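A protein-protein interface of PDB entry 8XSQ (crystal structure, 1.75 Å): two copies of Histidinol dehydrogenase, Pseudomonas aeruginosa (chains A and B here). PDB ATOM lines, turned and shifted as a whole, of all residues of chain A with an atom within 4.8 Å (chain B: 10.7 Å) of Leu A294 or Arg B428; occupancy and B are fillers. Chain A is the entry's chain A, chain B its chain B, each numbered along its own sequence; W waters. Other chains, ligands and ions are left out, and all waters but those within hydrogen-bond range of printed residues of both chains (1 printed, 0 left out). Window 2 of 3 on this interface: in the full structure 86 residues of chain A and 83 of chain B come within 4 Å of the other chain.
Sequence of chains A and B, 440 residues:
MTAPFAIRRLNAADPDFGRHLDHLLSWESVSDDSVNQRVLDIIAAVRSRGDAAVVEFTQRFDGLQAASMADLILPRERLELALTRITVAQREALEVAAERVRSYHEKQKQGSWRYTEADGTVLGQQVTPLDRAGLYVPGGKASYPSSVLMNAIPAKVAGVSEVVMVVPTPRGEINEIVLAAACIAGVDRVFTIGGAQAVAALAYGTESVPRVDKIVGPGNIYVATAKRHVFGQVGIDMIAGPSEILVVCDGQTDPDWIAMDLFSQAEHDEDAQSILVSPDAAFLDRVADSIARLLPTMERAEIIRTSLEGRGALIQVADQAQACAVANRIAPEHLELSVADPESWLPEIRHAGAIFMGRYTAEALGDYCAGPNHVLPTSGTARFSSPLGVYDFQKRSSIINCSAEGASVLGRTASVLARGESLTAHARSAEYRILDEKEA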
ATOM      1  N   ASP A 256      -7.693 -15.414  14.157  1.00  0.00           N
ATOM      2  CA  ASP A 256      -9.089 -15.836  14.232  1.00  0.00           C
ATOM      3  C   ASP A 256      -9.343 -16.636  15.503  1.00  0.00           C
ATOM      4  O   ASP A 256     -10.413 -16.520  16.114  1.00  0.00           O
ATOM      5  CB  ASP A 256      -9.464 -16.666  13.004  1.00  0.00           C
ATOM      6  CG  ASP A 256      -9.384 -15.874  11.715  1.00  0.00           C
ATOM      7  OD1 ASP A 256      -9.711 -14.668  11.720  1.00  0.00           O
ATOM      8  OD2 ASP A 256      -8.987 -16.471  10.690  1.00  0.00           O
ATOM      9  N   ALA A 259      -9.530 -13.997  18.333  1.00  0.00           N
ATOM     10  CA  ALA A 259     -10.807 -13.296  18.247  1.00  0.00           C
ATOM     11  C   ALA A 259     -11.942 -14.164  18.778  1.00  0.00           C
ATOM     12  O   ALA A 259     -12.782 -13.702  19.559  1.00  0.00           O
ATOM     13  CB  ALA A 259     -11.081 -12.869  16.803  1.00  0.00           C
ATOM     14  N   MET A 260     -11.967 -15.439  18.379  1.00  0.00           N
ATOM     15  CA  MET A 260     -13.018 -16.337  18.845  1.00  0.00           C
ATOM     16  C   MET A 260     -12.896 -16.634  20.334  1.00  0.00           C
ATOM     17  O   MET A 260     -13.917 -16.796  21.015  1.00  0.00           O
ATOM     18  CB  MET A 260     -13.003 -17.637  18.041  1.00  0.00           C
ATOM     19  CG  MET A 260     -14.286 -18.437  18.182  1.00  0.00           C
ATOM     20  SD  MET A 260     -15.716 -17.577  17.497  1.00  0.00           S
ATOM     21  CE  MET A 260     -15.101 -17.116  15.881  1.00  0.00           C
ATOM     22  N   PHE A 263     -14.568 -13.812  21.773  1.00  0.00           N
ATOM     23  CA  PHE A 263     -16.003 -13.979  21.564  1.00  0.00           C
ATOM     24  C   PHE A 263     -16.602 -14.985  22.538  1.00  0.00           C
ATOM     25  O   PHE A 263     -17.762 -14.843  22.941  1.00  0.00           O
ATOM     26  CB  PHE A 263     -16.291 -14.450  20.136  1.00  0.00           C
ATOM     27  CG  PHE A 263     -16.167 -13.377  19.083  1.00  0.00           C
ATOM     28  CD1 PHE A 263     -15.718 -12.107  19.393  1.00  0.00           C
ATOM     29  CD2 PHE A 263     -16.515 -13.658  17.770  1.00  0.00           C
ATOM     30  CE1 PHE A 263     -15.610 -11.132  18.411  1.00  0.00           C
ATOM     31  CE2 PHE A 263     -16.412 -12.692  16.783  1.00  0.00           C
ATOM     32  CZ  PHE A 263     -15.958 -11.426  17.106  1.00  0.00           C
ATOM     33  N   SER A 290     -10.035  -9.575  12.404  1.00  0.00           N
ATOM     34  CA  SER A 290     -10.754 -10.829  12.604  1.00  0.00           C
ATOM     35  C   SER A 290     -12.053 -10.604  13.364  1.00  0.00           C
ATOM     36  O   SER A 290     -13.080 -11.216  13.049  1.00  0.00           O
ATOM     37  CB  SER A 290      -9.868 -11.830  13.347  1.00  0.00           C
ATOM     38  OG  SER A 290      -8.790 -12.258  12.535  1.00  0.00           O
ATOM     39  N   ILE A 291     -12.025  -9.730  14.372  1.00  0.00           N
ATOM     40  CA  ILE A 291     -13.238  -9.420  15.125  1.00  0.00           C
ATOM     41  C   ILE A 291     -14.284  -8.804  14.205  1.00  0.00           C
ATOM     42  O   ILE A 291     -15.450  -9.216  14.194  1.00  0.00           O
ATOM     43  CB  ILE A 291     -12.912  -8.489  16.305  1.00  0.00           C
ATOM     44  CG1 ILE A 291     -12.191  -9.257  17.412  1.00  0.00           C
ATOM     45  CG2 ILE A 291     -14.185  -7.853  16.851  1.00  0.00           C
ATOM     46  CD1 ILE A 291     -11.659  -8.365  18.522  1.00  0.00           C
ATOM     47  N   ALA A 292     -13.876  -7.813  13.409  1.00  0.00           N
ATOM     48  CA  ALA A 292     -14.819  -7.123  12.535  1.00  0.00           C
ATOM     49  C   ALA A 292     -15.437  -8.075  11.518  1.00  0.00           C
ATOM     50  O   ALA A 292     -16.624  -7.960  11.190  1.00  0.00           O
ATOM     51  CB  ALA A 292     -14.123  -5.960  11.829  1.00  0.00           C
ATOM     52  N   ARG A 293     -14.651  -9.030  11.015  1.00  0.00           N
ATOM     53  CA  ARG A 293     -15.161  -9.957  10.011  1.00  0.00           C
ATOM     54  C   ARG A 293     -16.017 -11.055  10.633  1.00  0.00           C
ATOM     55  O   ARG A 293     -17.039 -11.449  10.059  1.00  0.00           O
ATOM     56  CB  ARG A 293     -14.001 -10.576   9.229  1.00  0.00           C
ATOM     57  CG  ARG A 293     -14.413 -11.699   8.289  1.00  0.00           C
ATOM     58  CD  ARG A 293     -13.279 -12.081   7.356  1.00  0.00           C
ATOM     59  NE  ARG A 293     -12.071 -12.440   8.090  1.00  0.00           N
ATOM     60  CZ  ARG A 293     -11.857 -13.621   8.651  1.00  0.00           C
ATOM     61  NH1 ARG A 293     -12.749 -14.595   8.572  1.00  0.00           N
ATOM     62  NH2 ARG A 293     -10.718 -13.833   9.306  1.00  0.00           N
ATOM     63  N   LEU A 294     -15.623 -11.559  11.805  1.00  0.00           N
ATOM     64  CA  LEU A 294     -16.301 -12.718  12.376  1.00  0.00           C
ATOM     65  C   LEU A 294     -17.555 -12.340  13.154  1.00  0.00           C
ATOM     66  O   LEU A 294     -18.468 -13.164  13.274  1.00  0.00           O
ATOM     67  CB  LEU A 294     -15.342 -13.490  13.284  1.00  0.00           C
ATOM     68  CG  LEU A 294     -14.223 -14.270  12.592  1.00  0.00           C
ATOM     69  CD1 LEU A 294     -13.181 -14.721  13.604  1.00  0.00           C
ATOM     70  CD2 LEU A 294     -14.777 -15.461  11.820  1.00  0.00           C
ATOM     71  N   LEU A 295     -17.622 -11.117  13.684  1.00  0.00           N
ATOM     72  CA  LEU A 295     -18.735 -10.745  14.559  1.00  0.00           C
ATOM     73  C   LEU A 295     -20.106 -10.921  13.913  1.00  0.00           C
ATOM     74  O   LEU A 295     -20.975 -11.553  14.539  1.00  0.00           O
ATOM     75  CB  LEU A 295     -18.536  -9.313  15.067  1.00  0.00           C
ATOM     76  CG  LEU A 295     -19.622  -8.746  15.986  1.00  0.00           C
ATOM     77  CD1 LEU A 295     -19.866  -9.658  17.174  1.00  0.00           C
ATOM     78  CD2 LEU A 295     -19.243  -7.348  16.459  1.00  0.00           C
ATOM     79  N   PRO A 296     -20.380 -10.416  12.702  1.00  0.00           N
ATOM     80  CA  PRO A 296     -21.734 -10.584  12.142  1.00  0.00           C
ATOM     81  C   PRO A 296     -22.091 -12.022  11.800  1.00  0.00           C
ATOM     82  O   PRO A 296     -23.266 -12.291  11.519  1.00  0.00           O
ATOM     83  CB  PRO A 296     -21.712  -9.705  10.886  1.00  0.00           C
ATOM     84  CG  PRO A 296     -20.280  -9.588  10.525  1.00  0.00           C
ATOM     85  CD  PRO A 296     -19.524  -9.605  11.816  1.00  0.00           C
ATOM     86  N   THR A 297     -21.137 -12.950  11.817  1.00  0.00           N
ATOM     87  CA  THR A 297     -21.446 -14.349  11.552  1.00  0.00           C
ATOM     88  C   THR A 297     -21.875 -15.116  12.798  1.00  0.00           C
ATOM     89  O   THR A 297     -22.263 -16.282  12.681  1.00  0.00           O
ATOM     90  CB  THR A 297     -20.239 -15.062  10.923  1.00  0.00           C
ATOM     91  OG1 THR A 297     -19.290 -15.410  11.943  1.00  0.00           O
ATOM     92  CG2 THR A 297     -19.568 -14.173   9.890  1.00  0.00           C
ATOM     93  N   MET A 298     -21.820 -14.501  13.976  1.00  0.00           N
ATOM     94  CA  MET A 298     -22.046 -15.224  15.217  1.00  0.00           C
ATOM     95  C   MET A 298     -23.516 -15.213  15.607  1.00  0.00           C
ATOM     96  O   MET A 298     -24.195 -14.188  15.504  1.00  0.00           O
ATOM     97  CB  MET A 298     -21.197 -14.629  16.343  1.00  0.00           C
ATOM     98  CG  MET A 298     -19.769 -14.368  15.917  1.00  0.00           C
ATOM     99  SD  MET A 298     -18.857 -15.890  15.620  1.00  0.00           S
ATOM    100  CE  MET A 298     -19.568 -17.002  16.838  1.00  0.00           C
ATOM    101  N   ALA B 407      -5.993 -31.115  23.025  1.00  0.00           N
ATOM    102  CA  ALA B 407      -6.987 -30.103  22.686  1.00  0.00           C
ATOM    103  C   ALA B 407      -7.994 -30.624  21.670  1.00  0.00           C
ATOM    104  O   ALA B 407      -9.150 -30.185  21.661  1.00  0.00           O
ATOM    105  CB  ALA B 407      -6.297 -28.852  22.148  1.00  0.00           C
ATOM    106  N   LEU B 410     -10.457 -32.991  23.798  1.00  0.00           N
ATOM    107  CA  LEU B 410     -11.346 -32.180  24.622  1.00  0.00           C
ATOM    108  C   LEU B 410     -12.219 -31.266  23.776  1.00  0.00           C
ATOM    109  O   LEU B 410     -13.354 -30.966  24.162  1.00  0.00           O
ATOM    110  CB  LEU B 410     -10.533 -31.355  25.619  1.00  0.00           C
ATOM    111  CG  LEU B 410      -9.732 -32.136  26.662  1.00  0.00           C
ATOM    112  CD1 LEU B 410      -8.940 -31.183  27.551  1.00  0.00           C
ATOM    113  CD2 LEU B 410     -10.640 -33.035  27.491  1.00  0.00           C
ATOM    114  N   GLY B 411     -11.712 -30.813  22.626  1.00  0.00           N
ATOM    115  CA  GLY B 411     -12.483 -29.914  21.788  1.00  0.00           C
ATOM    116  C   GLY B 411     -13.736 -30.548  21.222  1.00  0.00           C
ATOM    117  O   GLY B 411     -14.756 -29.872  21.056  1.00  0.00           O
ATOM    118  N   ARG B 412     -13.684 -31.846  20.915  1.00  0.00           N
ATOM    119  CA  ARG B 412     -14.871 -32.519  20.397  1.00  0.00           C
ATOM    120  C   ARG B 412     -15.977 -32.558  21.442  1.00  0.00           C
ATOM    121  O   ARG B 412     -17.153 -32.354  21.120  1.00  0.00           O
ATOM    122  CB  ARG B 412     -14.509 -33.928  19.928  1.00  0.00           C
ATOM    123  CG  ARG B 412     -13.609 -33.934  18.705  1.00  0.00           C
ATOM    124  CD  ARG B 412     -13.533 -35.301  18.045  1.00  0.00           C
ATOM    125  NE  ARG B 412     -12.596 -35.293  16.927  1.00  0.00           N
ATOM    126  CZ  ARG B 412     -11.294 -35.516  17.042  1.00  0.00           C
ATOM    127  NH1 ARG B 412     -10.738 -35.775  18.216  1.00  0.00           N
ATOM    128  NH2 ARG B 412     -10.530 -35.474  15.954  1.00  0.00           N
ATOM    129  N   THR B 413     -15.618 -32.803  22.704  1.00  0.00           N
ATOM    130  CA  THR B 413     -16.612 -32.782  23.770  1.00  0.00           C
ATOM    131  C   THR B 413     -17.141 -31.373  24.001  1.00  0.00           C
ATOM    132  O   THR B 413     -18.352 -31.176  24.154  1.00  0.00           O
ATOM    133  CB  THR B 413     -16.011 -33.350  25.056  1.00  0.00           C
ATOM    134  OG1 THR B 413     -15.731 -34.742  24.872  1.00  0.00           O
ATOM    135  CG2 THR B 413     -16.974 -33.177  26.223  1.00  0.00           C
ATOM    136  N   ALA B 414     -16.247 -30.381  24.023  1.00  0.00           N
ATOM    137  CA  ALA B 414     -16.684 -29.001  24.193  1.00  0.00           C
ATOM    138  C   ALA B 414     -17.584 -28.564  23.044  1.00  0.00           C
ATOM    139  O   ALA B 414     -18.583 -27.871  23.260  1.00  0.00           O
ATOM    140  CB  ALA B 414     -15.471 -28.079  24.311  1.00  0.00           C
ATOM    141  N   SER B 415     -17.246 -28.964  21.815  1.00  0.00           N
ATOM    142  CA  SER B 415     -18.087 -28.636  20.667  1.00  0.00           C
ATOM    143  C   SER B 415     -19.498 -29.189  20.840  1.00  0.00           C
ATOM    144  O   SER B 415     -20.484 -28.472  20.646  1.00  0.00           O
ATOM    145  CB  SER B 415     -17.451 -29.174  19.383  1.00  0.00           C
ATOM    146  OG  SER B 415     -18.312 -28.999  18.268  1.00  0.00           O
ATOM    147  N   VAL B 416     -19.611 -30.467  21.212  1.00  0.00           N
ATOM    148  CA  VAL B 416     -20.922 -31.106  21.343  1.00  0.00           C
ATOM    149  C   VAL B 416     -21.807 -30.327  22.311  1.00  0.00           C
ATOM    150  O   VAL B 416     -22.956 -29.989  21.998  1.00  0.00           O
ATOM    151  CB  VAL B 416     -20.757 -32.572  21.785  1.00  0.00           C
ATOM    152  CG1 VAL B 416     -22.082 -33.136  22.279  1.00  0.00           C
ATOM    153  CG2 VAL B 416     -20.224 -33.416  20.633  1.00  0.00           C
ATOM    154  N   LEU B 417     -21.285 -30.023  23.498  1.00  0.00           N
ATOM    155  CA  LEU B 417     -22.111 -29.376  24.512  1.00  0.00           C
ATOM    156  C   LEU B 417     -22.355 -27.906  24.184  1.00  0.00           C
ATOM    157  O   LEU B 417     -23.464 -27.398  24.387  1.00  0.00           O
ATOM    158  CB  LEU B 417     -21.462 -29.531  25.885  1.00  0.00           C
ATOM    159  CG  LEU B 417     -21.413 -30.966  26.414  1.00  0.00           C
ATOM    160  CD1 LEU B 417     -20.679 -31.032  27.750  1.00  0.00           C
ATOM    161  CD2 LEU B 417     -22.815 -31.551  26.537  1.00  0.00           C
ATOM    162  N   ALA B 418     -21.337 -27.206  23.675  1.00  0.00           N
ATOM    163  CA  ALA B 418     -21.520 -25.801  23.322  1.00  0.00           C
ATOM    164  C   ALA B 418     -22.515 -25.644  22.180  1.00  0.00           C
ATOM    165  O   ALA B 418     -23.397 -24.777  22.232  1.00  0.00           O
ATOM    166  CB  ALA B 418     -20.181 -25.164  22.956  1.00  0.00           C
ATOM    167  N   ARG B 419     -22.388 -26.467  21.136  1.00  0.00           N
ATOM    168  CA  ARG B 419     -23.349 -26.414  20.038  1.00  0.00           C
ATOM    169  C   ARG B 419     -24.754 -26.752  20.522  1.00  0.00           C
ATOM    170  O   ARG B 419     -25.732 -26.132  20.088  1.00  0.00           O
ATOM    171  CB  ARG B 419     -22.926 -27.360  18.912  1.00  0.00           C
ATOM    172  CG  ARG B 419     -21.620 -26.978  18.234  1.00  0.00           C
ATOM    173  CD  ARG B 419     -21.863 -26.449  16.839  1.00  0.00           C
ATOM    174  NE  ARG B 419     -20.676 -25.832  16.262  1.00  0.00           N
ATOM    175  CZ  ARG B 419     -20.701 -24.745  15.503  1.00  0.00           C
ATOM    176  NH1 ARG B 419     -21.838 -24.130  15.219  1.00  0.00           N
ATOM    177  NH2 ARG B 419     -19.559 -24.266  15.017  1.00  0.00           N
ATOM    178  N   GLY B 420     -24.875 -27.726  21.426  1.00  0.00           N
ATOM    179  CA  GLY B 420     -26.183 -28.060  21.968  1.00  0.00           C
ATOM    180  C   GLY B 420     -26.838 -26.903  22.699  1.00  0.00           C
ATOM    181  O   GLY B 420     -28.069 -26.819  22.760  1.00  0.00           O
ATOM    182  N   SER B 422     -26.206 -23.700  21.788  1.00  0.00           N
ATOM    183  CA  SER B 422     -26.099 -22.577  20.857  1.00  0.00           C
ATOM    184  C   SER B 422     -25.080 -21.532  21.309  1.00  0.00           C
ATOM    185  O   SER B 422     -25.172 -20.364  20.920  1.00  0.00           O
ATOM    186  CB  SER B 422     -27.463 -21.915  20.618  1.00  0.00           C
ATOM    187  OG  SER B 422     -28.437 -22.875  20.247  1.00  0.00           O
ATOM    188  N   LEU B 423     -24.102 -21.921  22.128  1.00  0.00           N
ATOM    189  CA  LEU B 423     -22.987 -21.031  22.468  1.00  0.00           C
ATOM    190  C   LEU B 423     -21.891 -21.272  21.436  1.00  0.00           C
ATOM    191  O   LEU B 423     -20.888 -21.944  21.686  1.00  0.00           O
ATOM    192  CB  LEU B 423     -22.494 -21.285  23.889  1.00  0.00           C
ATOM    193  CG  LEU B 423     -23.425 -21.001  25.076  1.00  0.00           C
ATOM    194  CD1 LEU B 423     -22.629 -20.573  26.306  1.00  0.00           C
ATOM    195  CD2 LEU B 423     -24.488 -19.964  24.741  1.00  0.00           C
ATOM    196  N   THR B 424     -22.100 -20.717  20.240  1.00  0.00           N
ATOM    197  CA  THR B 424     -21.283 -21.104  19.096  1.00  0.00           C
ATOM    198  C   THR B 424     -19.889 -20.491  19.110  1.00  0.00           C
ATOM    199  O   THR B 424     -18.992 -21.024  18.449  1.00  0.00           O
ATOM    200  CB  THR B 424     -21.994 -20.749  17.787  1.00  0.00           C
ATOM    201  OG1 THR B 424     -22.222 -19.337  17.724  1.00  0.00           O
ATOM    202  CG2 THR B 424     -23.327 -21.479  17.695  1.00  0.00           C
ATOM    203  N   ALA B 425     -19.672 -19.390  19.837  1.00  0.00           N
ATOM    204  CA  ALA B 425     -18.306 -18.895  19.970  1.00  0.00           C
ATOM    205  C   ALA B 425     -17.470 -19.841  20.820  1.00  0.00           C
ATOM    206  O   ALA B 425     -16.305 -20.108  20.499  1.00  0.00           O
ATOM    207  CB  ALA B 425     -18.294 -17.485  20.559  1.00  0.00           C
ATOM    208  N   HIS B 426     -18.049 -20.357  21.910  1.00  0.00           N
ATOM    209  CA  HIS B 426     -17.420 -21.445  22.653  1.00  0.00           C
ATOM    210  C   HIS B 426     -17.074 -22.604  21.727  1.00  0.00           C
ATOM    211  O   HIS B 426     -15.948 -23.120  21.741  1.00  0.00           O
ATOM    212  CB  HIS B 426     -18.355 -21.938  23.761  1.00  0.00           C
ATOM    213  CG  HIS B 426     -18.265 -21.168  25.042  1.00  0.00           C
ATOM    214  ND1 HIS B 426     -18.873 -19.945  25.221  1.00  0.00           N
ATOM    215  CD2 HIS B 426     -17.665 -21.467  26.219  1.00  0.00           C
ATOM    216  CE1 HIS B 426     -18.644 -19.519  26.451  1.00  0.00           C
ATOM    217  NE2 HIS B 426     -17.909 -20.421  27.075  1.00  0.00           N
ATOM    218  N   ALA B 427     -18.048 -23.037  20.923  1.00  0.00           N
ATOM    219  CA  ALA B 427     -17.848 -24.196  20.062  1.00  0.00           C
ATOM    220  C   ALA B 427     -16.750 -23.940  19.039  1.00  0.00           C
ATOM    221  O   ALA B 427     -15.835 -24.755  18.878  1.00  0.00           O
ATOM    222  CB  ALA B 427     -19.158 -24.558  19.362  1.00  0.00           C
ATOM    223  N   ARG B 428     -16.820 -22.805  18.341  1.00  0.00           N
ATOM    224  CA  ARG B 428     -15.839 -22.522  17.299  1.00  0.00           C
ATOM    225  C   ARG B 428     -14.448 -22.331  17.885  1.00  0.00           C
ATOM    226  O   ARG B 428     -13.449 -22.724  17.272  1.00  0.00           O
ATOM    227  CB  ARG B 428     -16.277 -21.294  16.500  1.00  0.00           C
ATOM    228  CG  ARG B 428     -17.514 -21.557  15.653  1.00  0.00           C
ATOM    229  CD  ARG B 428     -17.990 -20.313  14.922  1.00  0.00           C
ATOM    230  NE  ARG B 428     -17.129 -19.962  13.801  1.00  0.00           N
ATOM    231  CZ  ARG B 428     -17.325 -18.916  13.011  1.00  0.00           C
ATOM    232  NH1 ARG B 428     -18.355 -18.103  13.186  1.00  0.00           N
ATOM    233  NH2 ARG B 428     -16.469 -18.679  12.020  1.00  0.00           N
ATOM    234  N   SER B 429     -14.364 -21.746  19.081  1.00  0.00           N
ATOM    235  CA  SER B 429     -13.069 -21.579  19.733  1.00  0.00           C
ATOM    236  C   SER B 429     -12.421 -22.934  20.006  1.00  0.00           C
ATOM    237  O   SER B 429     -11.227 -23.128  19.750  1.00  0.00           O
ATOM    238  CB  SER B 429     -13.246 -20.774  21.022  1.00  0.00           C
ATOM    239  OG  SER B 429     -12.222 -21.047  21.953  1.00  0.00           O
ATOM    240  N   ALA B 430     -13.203 -23.895  20.504  1.00  0.00           N
ATOM    241  CA  ALA B 430     -12.674 -25.238  20.721  1.00  0.00           C
ATOM    242  C   ALA B 430     -12.425 -25.953  19.399  1.00  0.00           C
ATOM    243  O   ALA B 430     -11.428 -26.670  19.252  1.00  0.00           O
ATOM    244  CB  ALA B 430     -13.635 -26.050  21.591  1.00  0.00           C
ATOM    245  N   GLU B 431     -13.318 -25.761  18.423  1.00  0.00           N
ATOM    246  CA  GLU B 431     -13.208 -26.477  17.156  1.00  0.00           C
ATOM    247  C   GLU B 431     -11.985 -26.043  16.357  1.00  0.00           C
ATOM    248  O   GLU B 431     -11.464 -26.828  15.556  1.00  0.00           O
ATOM    249  CB  GLU B 431     -14.479 -26.276  16.331  1.00  0.00           C
ATOM    250  CG  GLU B 431     -15.678 -27.068  16.834  1.00  0.00           C
ATOM    251  CD  GLU B 431     -17.004 -26.463  16.401  1.00  0.00           C
ATOM    252  OE1 GLU B 431     -16.992 -25.500  15.605  1.00  0.00           O
ATOM    253  OE2 GLU B 431     -18.059 -26.947  16.865  1.00  0.00           O
ATOM    254  N   TYR B 432     -11.515 -24.807  16.556  1.00  0.00           N
ATOM    255  CA  TYR B 432     -10.310 -24.353  15.866  1.00  0.00           C
ATOM    256  C   TYR B 432      -9.122 -25.262  16.145  1.00  0.00           C
ATOM    257  O   TYR B 432      -8.233 -25.398  15.297  1.00  0.00           O
ATOM    258  CB  TYR B 432      -9.959 -22.924  16.281  1.00  0.00           C
ATOM    259  CG  TYR B 432     -10.644 -21.831  15.492  1.00  0.00           C
ATOM    260  CD1 TYR B 432     -10.700 -21.871  14.105  1.00  0.00           C
ATOM    261  CD2 TYR B 432     -11.200 -20.734  16.136  1.00  0.00           C
ATOM    262  CE1 TYR B 432     -11.316 -20.859  13.386  1.00  0.00           C
ATOM    263  CE2 TYR B 432     -11.816 -19.723  15.428  1.00  0.00           C
ATOM    264  CZ  TYR B 432     -11.873 -19.788  14.057  1.00  0.00           C
ATOM    265  OH  TYR B 432     -12.490 -18.774  13.361  1.00  0.00           O
ATOM    266  N   ARG B 433      -9.086 -25.890  17.319  1.00  0.00           N
ATOM    267  CA  ARG B 433      -7.940 -26.685  17.738  1.00  0.00           C
ATOM    268  C   ARG B 433      -8.125 -28.176  17.494  1.00  0.00           C
ATOM    269  O   ARG B 433      -7.233 -28.960  17.836  1.00  0.00           O
ATOM    270  CB  ARG B 433      -7.642 -26.434  19.221  1.00  0.00           C
ATOM    271  CG  ARG B 433      -6.830 -25.167  19.485  1.00  0.00           C
ATOM    272  CD  ARG B 433      -7.744 -23.958  19.672  1.00  0.00           C
ATOM    273  NE  ARG B 433      -7.058 -22.831  20.292  1.00  0.00           N
ATOM    274  CZ  ARG B 433      -7.644 -21.684  20.608  1.00  0.00           C
ATOM    275  NH1 ARG B 433      -8.939 -21.491  20.404  1.00  0.00           N
ATOM    276  NH2 ARG B 433      -6.916 -20.706  21.142  1.00  0.00           N
ATOM    277  N   ILE B 434      -9.255 -28.590  16.918  1.00  0.00           N
ATOM    278  CA  ILE B 434      -9.457 -30.000  16.607  1.00  0.00           C
ATOM    279  C   ILE B 434      -8.573 -30.382  15.427  1.00  0.00           C
ATOM    280  O   ILE B 434      -8.519 -29.672  14.414  1.00  0.00           O
ATOM    281  CB  ILE B 434     -10.940 -30.283  16.323  1.00  0.00           C
ATOM    282  CG1 ILE B 434     -11.756 -30.183  17.612  1.00  0.00           C
ATOM    283  CG2 ILE B 434     -11.119 -31.659  15.694  1.00  0.00           C
ATOM    284  CD1 ILE B 434     -13.242 -30.371  17.403  1.00  0.00           C
ATOM    285  N   LEU B 435      -7.873 -31.504  15.557  1.00  0.00           N
ATOM    286  CA  LEU B 435      -6.867 -31.924  14.595  1.00  0.00           C
ATOM    287  C   LEU B 435      -7.427 -32.933  13.600  1.00  0.00           C
ATOM    288  O   LEU B 435      -8.324 -33.719  13.916  1.00  0.00           O
ATOM    289  CB  LEU B 435      -5.658 -32.534  15.307  1.00  0.00           C
ATOM    290  CG  LEU B 435      -4.582 -31.565  15.793  1.00  0.00           C
ATOM    291  CD1 LEU B 435      -3.272 -32.304  16.013  1.00  0.00           C
ATOM    292  CD2 LEU B 435      -4.400 -30.421  14.804  1.00  0.00           C
HETATM  293  O   HOH W   1     -22.315 -18.861  14.990  1.00  0.00           O
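The side-chain hydroxyl (OG1) of Thr A297 lies within hydrogen-bond range of the guanidinium group (NH1) of Arg B428, 3.1 Å away. The side-chain sulfur of Met A298 sits at hydrogen-bond distance from the guanidinium group of Arg B428, 3.3 Å away.
Water W1 lies within hydrogen-bond range of OG1 of Thr B424 and O of Thr A297.
Tyr B432 touches Asp A256 (CE2 to O, 3.6 Å). Ala B425 touches Met A260. Arg B428 touches Met A260. Met A260 touches Ser B429. Tyr B432 touches Met A260. Phe A263 touches Ala B425 (O to CB, 3.6 Å). Arg B428 touches Leu A294 (NH2 to CD2, 3.6 Å). OG1 of Thr B424 touches CE of Met A298 (3.6 Å). CE of Met A298 touches N of Ala B425, 3.8 Å away.
No position is printed for both chains.
Of the 26 printed residues of chain B, 5 touch a printed residue of chain A. Printed residues of chain B that touch a printed residue of chain A: Thr B424, Ala B425, Arg B428, Ser B429 and Tyr B432. Among the printed residues, 11 pairs touch across the chains. Among the printed residues, no Asp or Glu carboxylate lies within 4 Å of a Lys or Arg side-chain nitrogen of the other chain.
Leu A294 touches just one residue of chain B: Arg B428 (3.6 Å). Of chain A, only Met A260 (3.9 Å), Leu A294 (3.6 Å), Thr A297 (3.1 Å) and Met A298 (3.3 Å) come within 4 Å of Arg B428. Of chain B, only Tyr B432 (3.6 Å) comes within 4 Å of Asp A256. No residue of chain B comes within 4 Å of Ser A290. Ala A292 touches none of the printed residues of chain B. No residue of chain B comes within 4 Å of Pro A296. Printed residues of chain B within 4 Å of Thr A297: Arg B428 (3.1 Å). Of the printed residues of chain B, Met A298 touches Thr B424, Ala B425 and Arg B428. Printed residues of chain A within 4 Å of Tyr B432: Asp A256 (3.6 Å) and Met A260 (3.5 Å). Printed residues of chain B within 4 Å of Phe A263: Ala B425 (3.6 Å). Printed residues of chain A within 4 Å of Thr B424: Met A298 (3.6 Å). The nearest residue of chain B that does not touch Leu A294 is Tyr B432 (4.1 Å). The nearest printed residue of chain A that does not touch Arg B428 is Arg A293 (6.5 Å). The nearest printed residue of chain A that does not touch Ala B425 is Ala A259 (6.8 Å).
The side-chain carboxylate (OD1) of Asp A256 lies within hydrogen-bond range of the side-chain hydroxyl (OG) of Ser A290 (2.7 Å). The side-chain carboxylate (OD1) of Asp A256 is in salt-bridge range of the guanidinium group (NH2) of Arg A293 (2.7 Å). The backbone carbonyl oxygen of Leu A294 lies within hydrogen-bond range of the side-chain hydroxyl of Thr A297. The side-chain hydroxyl (OG1) of Thr A297 sits at hydrogen-bond distance from the side-chain sulfur (SD) of Met A298, at 3.7 Å. The backbone carbonyl oxygen (O) of Ser B429 is in hydrogen-bond range of the guanidinium group (NH1) of Arg B433, 2.9 Å away.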
